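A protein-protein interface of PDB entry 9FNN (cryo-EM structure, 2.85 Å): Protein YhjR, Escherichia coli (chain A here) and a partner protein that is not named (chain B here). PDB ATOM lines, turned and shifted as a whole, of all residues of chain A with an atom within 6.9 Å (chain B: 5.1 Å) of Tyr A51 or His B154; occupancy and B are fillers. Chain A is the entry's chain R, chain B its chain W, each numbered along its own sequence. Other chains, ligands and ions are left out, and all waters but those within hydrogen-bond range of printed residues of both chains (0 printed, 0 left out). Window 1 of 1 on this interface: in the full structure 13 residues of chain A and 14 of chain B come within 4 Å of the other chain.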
ATOM      1  N   ILE A  49      -5.960 -28.668 -10.740  1.00  0.00           N
ATOM      2  CA  ILE A  49      -4.799 -29.000 -11.555  1.00  0.00           C
ATOM      3  C   ILE A  49      -3.923 -29.963 -10.769  1.00  0.00           C
ATOM      4  O   ILE A  49      -3.553 -29.679  -9.624  1.00  0.00           O
ATOM      5  CB  ILE A  49      -4.008 -27.741 -11.952  1.00  0.00           C
ATOM      6  CG1 ILE A  49      -4.824 -26.892 -12.924  1.00  0.00           C
ATOM      7  CG2 ILE A  49      -2.673 -28.122 -12.562  1.00  0.00           C
ATOM      8  CD1 ILE A  49      -5.197 -27.618 -14.188  1.00  0.00           C
ATOM      9  N   ASP A  50      -3.594 -31.096 -11.382  1.00  0.00           N
ATOM     10  CA  ASP A  50      -2.774 -32.132 -10.760  1.00  0.00           C
ATOM     11  C   ASP A  50      -1.562 -32.374 -11.654  1.00  0.00           C
ATOM     12  O   ASP A  50      -1.593 -33.227 -12.544  1.00  0.00           O
ATOM     13  CB  ASP A  50      -3.577 -33.410 -10.544  1.00  0.00           C
ATOM     14  CG  ASP A  50      -2.765 -34.503  -9.878  1.00  0.00           C
ATOM     15  OD1 ASP A  50      -2.366 -34.318  -8.709  1.00  0.00           O
ATOM     16  OD2 ASP A  50      -2.525 -35.545 -10.521  1.00  0.00           O
ATOM     17  N   TYR A  51      -0.496 -31.615 -11.415  1.00  0.00           N
ATOM     18  CA  TYR A  51       0.746 -31.752 -12.160  1.00  0.00           C
ATOM     19  C   TYR A  51       1.765 -32.638 -11.458  1.00  0.00           C
ATOM     20  O   TYR A  51       2.886 -32.781 -11.954  1.00  0.00           O
ATOM     21  CB  TYR A  51       1.355 -30.374 -12.430  1.00  0.00           C
ATOM     22  CG  TYR A  51       0.776 -29.691 -13.645  1.00  0.00           C
ATOM     23  CD1 TYR A  51       0.364 -30.426 -14.744  1.00  0.00           C
ATOM     24  CD2 TYR A  51       0.637 -28.313 -13.691  1.00  0.00           C
ATOM     25  CE1 TYR A  51      -0.167 -29.810 -15.855  1.00  0.00           C
ATOM     26  CE2 TYR A  51       0.107 -27.689 -14.798  1.00  0.00           C
ATOM     27  CZ  TYR A  51      -0.293 -28.442 -15.876  1.00  0.00           C
ATOM     28  OH  TYR A  51      -0.822 -27.823 -16.984  1.00  0.00           O
ATOM     29  N   ALA A  52       1.409 -33.228 -10.321  1.00  0.00           N
ATOM     30  CA  ALA A  52       2.310 -34.149  -9.647  1.00  0.00           C
ATOM     31  C   ALA A  52       2.430 -35.446 -10.436  1.00  0.00           C
ATOM     32  O   ALA A  52       1.454 -35.929 -11.016  1.00  0.00           O
ATOM     33  CB  ALA A  52       1.815 -34.437  -8.229  1.00  0.00           C
ATOM     34  N   ASP A  53       3.639 -36.009 -10.448  1.00  0.00           N
ATOM     35  CA  ASP A  53       3.933 -37.242 -11.180  1.00  0.00           C
ATOM     36  C   ASP A  53       3.592 -37.101 -12.661  1.00  0.00           C
ATOM     37  O   ASP A  53       3.040 -38.011 -13.281  1.00  0.00           O
ATOM     38  CB  ASP A  53       3.204 -38.439 -10.565  1.00  0.00           C
ATOM     39  CG  ASP A  53       3.527 -38.626  -9.096  1.00  0.00           C
ATOM     40  OD1 ASP A  53       4.644 -38.252  -8.679  1.00  0.00           O
ATOM     41  OD2 ASP A  53       2.665 -39.147  -8.357  1.00  0.00           O
ATOM     42  N   ILE A  54       3.926 -35.944 -13.235  1.00  0.00           N
ATOM     43  CA  ILE A  54       3.652 -35.697 -14.646  1.00  0.00           C
ATOM     44  C   ILE A  54       4.789 -36.158 -15.551  1.00  0.00           C
ATOM     45  O   ILE A  54       4.585 -36.292 -16.766  1.00  0.00           O
ATOM     46  CB  ILE A  54       3.369 -34.204 -14.887  1.00  0.00           C
ATOM     47  CG1 ILE A  54       2.432 -34.015 -16.080  1.00  0.00           C
ATOM     48  CG2 ILE A  54       4.665 -33.433 -15.096  1.00  0.00           C
ATOM     49  CD1 ILE A  54       0.979 -34.240 -15.746  1.00  0.00           C
ATOM     50  N   SER A  55       5.972 -36.417 -14.997  1.00  0.00           N
ATOM     51  CA  SER A  55       7.144 -36.793 -15.773  1.00  0.00           C
ATOM     52  C   SER A  55       7.311 -38.301 -15.902  1.00  0.00           C
ATOM     53  O   SER A  55       8.333 -38.757 -16.424  1.00  0.00           O
ATOM     54  CB  SER A  55       8.403 -36.186 -15.151  1.00  0.00           C
ATOM     55  OG  SER A  55       8.319 -34.773 -15.106  1.00  0.00           O
ATOM     56  N   LEU A  69       5.564 -23.904 -23.634  1.00  0.00           N
ATOM     57  CA  LEU A  69       4.440 -23.408 -22.844  1.00  0.00           C
ATOM     58  C   LEU A  69       3.918 -24.480 -21.894  1.00  0.00           C
ATOM     59  O   LEU A  69       3.715 -24.224 -20.697  1.00  0.00           O
ATOM     60  CB  LEU A  69       3.330 -22.920 -23.774  1.00  0.00           C
ATOM     61  CG  LEU A  69       2.216 -22.066 -23.172  1.00  0.00           C
ATOM     62  CD1 LEU A  69       2.757 -20.730 -22.713  1.00  0.00           C
ATOM     63  CD2 LEU A  69       1.109 -21.874 -24.184  1.00  0.00           C
ATOM     64  N   LEU A  70       3.698 -25.691 -22.410  1.00  0.00           N
ATOM     65  CA  LEU A  70       3.225 -26.783 -21.567  1.00  0.00           C
ATOM     66  C   LEU A  70       4.236 -27.107 -20.478  1.00  0.00           C
ATOM     67  O   LEU A  70       3.864 -27.338 -19.322  1.00  0.00           O
ATOM     68  CB  LEU A  70       2.941 -28.019 -22.419  1.00  0.00           C
ATOM     69  CG  LEU A  70       2.182 -27.804 -23.727  1.00  0.00           C
ATOM     70  CD1 LEU A  70       2.009 -29.119 -24.459  1.00  0.00           C
ATOM     71  CD2 LEU A  70       0.838 -27.152 -23.479  1.00  0.00           C
ATOM     72  N   ALA A  71       5.523 -27.130 -20.830  1.00  0.00           N
ATOM     73  CA  ALA A  71       6.559 -27.390 -19.838  1.00  0.00           C
ATOM     74  C   ALA A  71       6.580 -26.308 -18.769  1.00  0.00           C
ATOM     75  O   ALA A  71       6.701 -26.606 -17.576  1.00  0.00           O
ATOM     76  CB  ALA A  71       7.921 -27.499 -20.517  1.00  0.00           C
ATOM     77  N   GLU A  72       6.457 -25.046 -19.178  1.00  0.00           N
ATOM     78  CA  GLU A  72       6.453 -23.947 -18.220  1.00  0.00           C
ATOM     79  C   GLU A  72       5.281 -24.060 -17.259  1.00  0.00           C
ATOM     80  O   GLU A  72       5.414 -23.769 -16.065  1.00  0.00           O
ATOM     81  CB  GLU A  72       6.415 -22.615 -18.965  1.00  0.00           C
ATOM     82  CG  GLU A  72       5.953 -21.438 -18.136  1.00  0.00           C
ATOM     83  CD  GLU A  72       5.884 -20.163 -18.947  1.00  0.00           C
ATOM     84  OE1 GLU A  72       6.946 -19.683 -19.394  1.00  0.00           O
ATOM     85  OE2 GLU A  72       4.766 -19.649 -19.155  1.00  0.00           O
ATOM     86  N   PHE A  73       4.121 -24.479 -17.762  1.00  0.00           N
ATOM     87  CA  PHE A  73       2.976 -24.646 -16.873  1.00  0.00           C
ATOM     88  C   PHE A  73       3.122 -25.872 -15.981  1.00  0.00           C
ATOM     89  O   PHE A  73       2.629 -25.869 -14.848  1.00  0.00           O
ATOM     90  CB  PHE A  73       1.687 -24.720 -17.690  1.00  0.00           C
ATOM     91  CG  PHE A  73       1.213 -23.385 -18.181  1.00  0.00           C
ATOM     92  CD1 PHE A  73       1.126 -22.311 -17.317  1.00  0.00           C
ATOM     93  CD2 PHE A  73       0.881 -23.196 -19.509  1.00  0.00           C
ATOM     94  CE1 PHE A  73       0.701 -21.084 -17.761  1.00  0.00           C
ATOM     95  CE2 PHE A  73       0.456 -21.966 -19.960  1.00  0.00           C
ATOM     96  CZ  PHE A  73       0.366 -20.909 -19.082  1.00  0.00           C
ATOM     97  N   ALA A  74       3.806 -26.915 -16.454  1.00  0.00           N
ATOM     98  CA  ALA A  74       3.871 -28.176 -15.726  1.00  0.00           C
ATOM     99  C   ALA A  74       4.929 -28.199 -14.629  1.00  0.00           C
ATOM    100  O   ALA A  74       5.003 -29.186 -13.891  1.00  0.00           O
ATOM    101  CB  ALA A  74       4.126 -29.331 -16.695  1.00  0.00           C
ATOM    102  N   GLN A  75       5.744 -27.159 -14.498  1.00  0.00           N
ATOM    103  CA  GLN A  75       6.741 -27.117 -13.433  1.00  0.00           C
ATOM    104  C   GLN A  75       6.131 -26.595 -12.140  1.00  0.00           C
ATOM    105  O   GLN A  75       4.933 -26.745 -11.906  1.00  0.00           O
ATOM    106  CB  GLN A  75       7.934 -26.250 -13.836  1.00  0.00           C
ATOM    107  CG  GLN A  75       8.622 -26.693 -15.115  1.00  0.00           C
ATOM    108  CD  GLN A  75       9.109 -28.129 -15.059  1.00  0.00           C
ATOM    109  OE1 GLN A  75       9.506 -28.624 -14.005  1.00  0.00           O
ATOM    110  NE2 GLN A  75       9.080 -28.805 -16.201  1.00  0.00           N
ATOM    111  N   ASP B 150      -6.396 -25.642 -27.627  1.00  0.00           N
ATOM    112  CA  ASP B 150      -5.395 -24.771 -28.218  1.00  0.00           C
ATOM    113  C   ASP B 150      -4.628 -24.093 -27.095  1.00  0.00           C
ATOM    114  O   ASP B 150      -4.945 -24.252 -25.916  1.00  0.00           O
ATOM    115  CB  ASP B 150      -6.033 -23.747 -29.158  1.00  0.00           C
ATOM    116  CG  ASP B 150      -6.971 -22.802 -28.441  1.00  0.00           C
ATOM    117  OD1 ASP B 150      -7.542 -23.197 -27.405  1.00  0.00           O
ATOM    118  OD2 ASP B 150      -7.139 -21.659 -28.914  1.00  0.00           O
ATOM    119  N   ALA B 151      -3.606 -23.330 -27.483  1.00  0.00           N
ATOM    120  CA  ALA B 151      -2.741 -22.693 -26.499  1.00  0.00           C
ATOM    121  C   ALA B 151      -3.500 -21.671 -25.664  1.00  0.00           C
ATOM    122  O   ALA B 151      -3.261 -21.545 -24.459  1.00  0.00           O
ATOM    123  CB  ALA B 151      -1.551 -22.038 -27.196  1.00  0.00           C
ATOM    124  N   ASN B 152      -4.421 -20.933 -26.289  1.00  0.00           N
ATOM    125  CA  ASN B 152      -5.130 -19.871 -25.585  1.00  0.00           C
ATOM    126  C   ASN B 152      -5.924 -20.420 -24.405  1.00  0.00           C
ATOM    127  O   ASN B 152      -5.824 -19.909 -23.282  1.00  0.00           O
ATOM    128  CB  ASN B 152      -6.047 -19.133 -26.559  1.00  0.00           C
ATOM    129  CG  ASN B 152      -6.747 -17.956 -25.924  1.00  0.00           C
ATOM    130  OD1 ASN B 152      -7.768 -18.110 -25.257  1.00  0.00           O
ATOM    131  ND2 ASN B 152      -6.210 -16.765 -26.142  1.00  0.00           N
ATOM    132  N   CYS B 153      -6.708 -21.474 -24.635  1.00  0.00           N
ATOM    133  CA  CYS B 153      -7.495 -22.052 -23.553  1.00  0.00           C
ATOM    134  C   CYS B 153      -6.611 -22.727 -22.514  1.00  0.00           C
ATOM    135  O   CYS B 153      -6.934 -22.706 -21.321  1.00  0.00           O
ATOM    136  CB  CYS B 153      -8.516 -23.039 -24.111  1.00  0.00           C
ATOM    137  SG  CYS B 153      -9.821 -22.274 -25.100  1.00  0.00           S
ATOM    138  N   HIS B 154      -5.497 -23.321 -22.945  1.00  0.00           N
ATOM    139  CA  HIS B 154      -4.562 -23.912 -21.996  1.00  0.00           C
ATOM    140  C   HIS B 154      -4.009 -22.861 -21.045  1.00  0.00           C
ATOM    141  O   HIS B 154      -3.897 -23.103 -19.838  1.00  0.00           O
ATOM    142  CB  HIS B 154      -3.429 -24.612 -22.743  1.00  0.00           C
ATOM    143  CG  HIS B 154      -2.415 -25.247 -21.844  1.00  0.00           C
ATOM    144  ND1 HIS B 154      -2.688 -26.363 -21.084  1.00  0.00           N
ATOM    145  CD2 HIS B 154      -1.127 -24.923 -21.584  1.00  0.00           C
ATOM    146  CE1 HIS B 154      -1.614 -26.697 -20.394  1.00  0.00           C
ATOM    147  NE2 HIS B 154      -0.652 -25.840 -20.680  1.00  0.00           N
ATOM    148  N   ILE B 155      -3.655 -21.687 -21.567  1.00  0.00           N
ATOM    149  CA  ILE B 155      -3.195 -20.608 -20.699  1.00  0.00           C
ATOM    150  C   ILE B 155      -4.327 -20.115 -19.810  1.00  0.00           C
ATOM    151  O   ILE B 155      -4.132 -19.868 -18.614  1.00  0.00           O
ATOM    152  CB  ILE B 155      -2.601 -19.459 -21.529  1.00  0.00           C
ATOM    153  CG1 ILE B 155      -1.511 -19.975 -22.458  1.00  0.00           C
ATOM    154  CG2 ILE B 155      -2.026 -18.409 -20.609  1.00  0.00           C
ATOM    155  CD1 ILE B 155      -1.220 -19.051 -23.610  1.00  0.00           C
ATOM    156  N   ARG B 156      -5.525 -19.956 -20.376  1.00  0.00           N
ATOM    157  CA  ARG B 156      -6.627 -19.376 -19.617  1.00  0.00           C
ATOM    158  C   ARG B 156      -7.057 -20.265 -18.460  1.00  0.00           C
ATOM    159  O   ARG B 156      -7.448 -19.756 -17.406  1.00  0.00           O
ATOM    160  CB  ARG B 156      -7.811 -19.097 -20.537  1.00  0.00           C
ATOM    161  CG  ARG B 156      -7.627 -17.890 -21.431  1.00  0.00           C
ATOM    162  CD  ARG B 156      -8.877 -17.634 -22.237  1.00  0.00           C
ATOM    163  NE  ARG B 156      -8.752 -16.453 -23.078  1.00  0.00           N
ATOM    164  CZ  ARG B 156      -9.190 -15.249 -22.743  1.00  0.00           C
ATOM    165  NH1 ARG B 156      -9.781 -15.028 -21.583  1.00  0.00           N
ATOM    166  NH2 ARG B 156      -9.034 -14.243 -23.595  1.00  0.00           N
ATOM    167  N   LEU B 157      -6.991 -21.585 -18.628  1.00  0.00           N
ATOM    168  CA  LEU B 157      -7.362 -22.487 -17.545  1.00  0.00           C
ATOM    169  C   LEU B 157      -6.425 -22.389 -16.349  1.00  0.00           C
ATOM    170  O   LEU B 157      -6.754 -22.915 -15.282  1.00  0.00           O
ATOM    171  CB  LEU B 157      -7.411 -23.927 -18.050  1.00  0.00           C
ATOM    172  CG  LEU B 157      -8.574 -24.243 -18.989  1.00  0.00           C
ATOM    173  CD1 LEU B 157      -8.533 -25.686 -19.435  1.00  0.00           C
ATOM    174  CD2 LEU B 157      -9.893 -23.927 -18.318  1.00  0.00           C
ATOM    175  N   HIS B 158      -5.275 -21.737 -16.497  1.00  0.00           N
ATOM    176  CA  HIS B 158      -4.321 -21.575 -15.413  1.00  0.00           C
ATOM    177  C   HIS B 158      -4.318 -20.176 -14.815  1.00  0.00           C
ATOM    178  O   HIS B 158      -3.557 -19.927 -13.876  1.00  0.00           O
ATOM    179  CB  HIS B 158      -2.909 -21.921 -15.896  1.00  0.00           C
ATOM    180  CG  HIS B 158      -2.748 -23.343 -16.328  1.00  0.00           C
ATOM    181  ND1 HIS B 158      -3.068 -23.778 -17.595  1.00  0.00           N
ATOM    182  CD2 HIS B 158      -2.301 -24.430 -15.659  1.00  0.00           C
ATOM    183  CE1 HIS B 158      -2.826 -25.073 -17.688  1.00  0.00           C
ATOM    184  NE2 HIS B 158      -2.361 -25.493 -16.527  1.00  0.00           N
ATOM    185  N   ILE B 183      -1.771 -31.200 -26.199  1.00  0.00           N
ATOM    186  CA  ILE B 183      -2.543 -30.503 -25.175  1.00  0.00           C
ATOM    187  C   ILE B 183      -3.663 -31.394 -24.656  1.00  0.00           C
ATOM    188  O   ILE B 183      -3.979 -31.387 -23.461  1.00  0.00           O
ATOM    189  CB  ILE B 183      -3.079 -29.168 -25.722  1.00  0.00           C
ATOM    190  CG1 ILE B 183      -1.922 -28.249 -26.104  1.00  0.00           C
ATOM    191  CG2 ILE B 183      -3.964 -28.483 -24.698  1.00  0.00           C
ATOM    192  CD1 ILE B 183      -2.356 -26.941 -26.691  1.00  0.00           C
ATOM    193  N   LEU B 186      -2.223 -33.984 -22.278  1.00  0.00           N
ATOM    194  CA  LEU B 186      -1.884 -33.313 -21.029  1.00  0.00           C
ATOM    195  C   LEU B 186      -3.133 -33.024 -20.204  1.00  0.00           C
ATOM    196  O   LEU B 186      -3.123 -33.173 -18.978  1.00  0.00           O
ATOM    197  CB  LEU B 186      -1.112 -32.031 -21.329  1.00  0.00           C
ATOM    198  CG  LEU B 186      -0.563 -31.232 -20.152  1.00  0.00           C
ATOM    199  CD1 LEU B 186       0.224 -32.125 -19.214  1.00  0.00           C
ATOM    200  CD2 LEU B 186       0.306 -30.101 -20.660  1.00  0.00           C
ATOM    201  N   TRP B 187      -4.221 -32.614 -20.860  1.00  0.00           N
ATOM    202  CA  TRP B 187      -5.470 -32.371 -20.145  1.00  0.00           C
ATOM    203  C   TRP B 187      -6.060 -33.662 -19.592  1.00  0.00           C
ATOM    204  O   TRP B 187      -6.565 -33.683 -18.464  1.00  0.00           O
ATOM    205  CB  TRP B 187      -6.479 -31.683 -21.061  1.00  0.00           C
ATOM    206  CG  TRP B 187      -6.185 -30.245 -21.318  1.00  0.00           C
ATOM    207  CD1 TRP B 187      -5.124 -29.530 -20.859  1.00  0.00           C
ATOM    208  CD2 TRP B 187      -6.974 -29.339 -22.093  1.00  0.00           C
ATOM    209  NE1 TRP B 187      -5.197 -28.236 -21.303  1.00  0.00           N
ATOM    210  CE2 TRP B 187      -6.327 -28.094 -22.062  1.00  0.00           C
ATOM    211  CE3 TRP B 187      -8.165 -29.462 -22.813  1.00  0.00           C
ATOM    212  CZ2 TRP B 187      -6.828 -26.979 -22.723  1.00  0.00           C
ATOM    213  CZ3 TRP B 187      -8.660 -28.356 -23.467  1.00  0.00           C
ATOM    214  CH2 TRP B 187      -7.993 -27.132 -23.418  1.00  0.00           C
ATOM    215  N   SER B 190      -4.231 -34.360 -16.576  1.00  0.00           N
ATOM    216  CA  SER B 190      -4.094 -33.307 -15.573  1.00  0.00           C
ATOM    217  C   SER B 190      -5.407 -32.650 -15.171  1.00  0.00           C
ATOM    218  O   SER B 190      -5.577 -32.313 -13.998  1.00  0.00           O
ATOM    219  CB  SER B 190      -3.125 -32.235 -16.085  1.00  0.00           C
ATOM    220  OG  SER B 190      -3.009 -31.176 -15.154  1.00  0.00           O
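The side-chain hydroxyl (OH) of Tyr A51 lies within hydrogen-bond range of a ring nitrogen (NE2) of His B158 (2.8 Å).
Of chain B, only His B154, His B158 and Ser B190 come within 4 Å of Tyr A51. His B154 touches just these residues of chain A: Tyr A51 (3.7 Å), Leu A70 (3.4 Å) and Phe A73 (3.3 Å). Of the printed residues of chain A, Leu B186 touches Leu A70 (3.8 Å). Of the printed residues of chain A, Ser B190 touches Asp A50 and Tyr A51. The nearest residue of chain B that does not touch Tyr A51 is Leu B186 (4.1 Å). The nearest printed residue of chain A that does not touch Leu B186 is Tyr A51 (4.1 Å).
The backbone carbonyl oxygen (O) of His B154 lies within hydrogen-bond range of a ring nitrogen (ND1) of His B158 (2.5 Å). A ring nitrogen (ND1) of His B154 is in hydrogen-bond range of the indole nitrogen of Trp B187 (3.1 Å).
Hydrophobic or aromatic side chains of chain A that line the printed part of chain B: Tyr A51, Leu A69, Leu A70 and Phe A73. Of the 13 printed residues of chain B, 6 touch a printed residue of chain A. Among the printed residues, 10 pairs touch across the chains.
Asp A50 touches Ser B190 (N to O, 3.5 Å). OH of Tyr A51 touches CE1 of His B154, 3.7 Å away. Tyr A51 touches Ser B190 (CE1 to OG, 3.2 Å). Ile B155 touches Leu A69. Leu A70 touches His B154. CG1 of Ile B183 touches CD2 of Leu A70, at 3.96 Å. CB of Leu A70 touches CD2 of Leu B186, 3.8 Å away. Phe A73 touches His B154. Phe A73 touches Ile B155.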
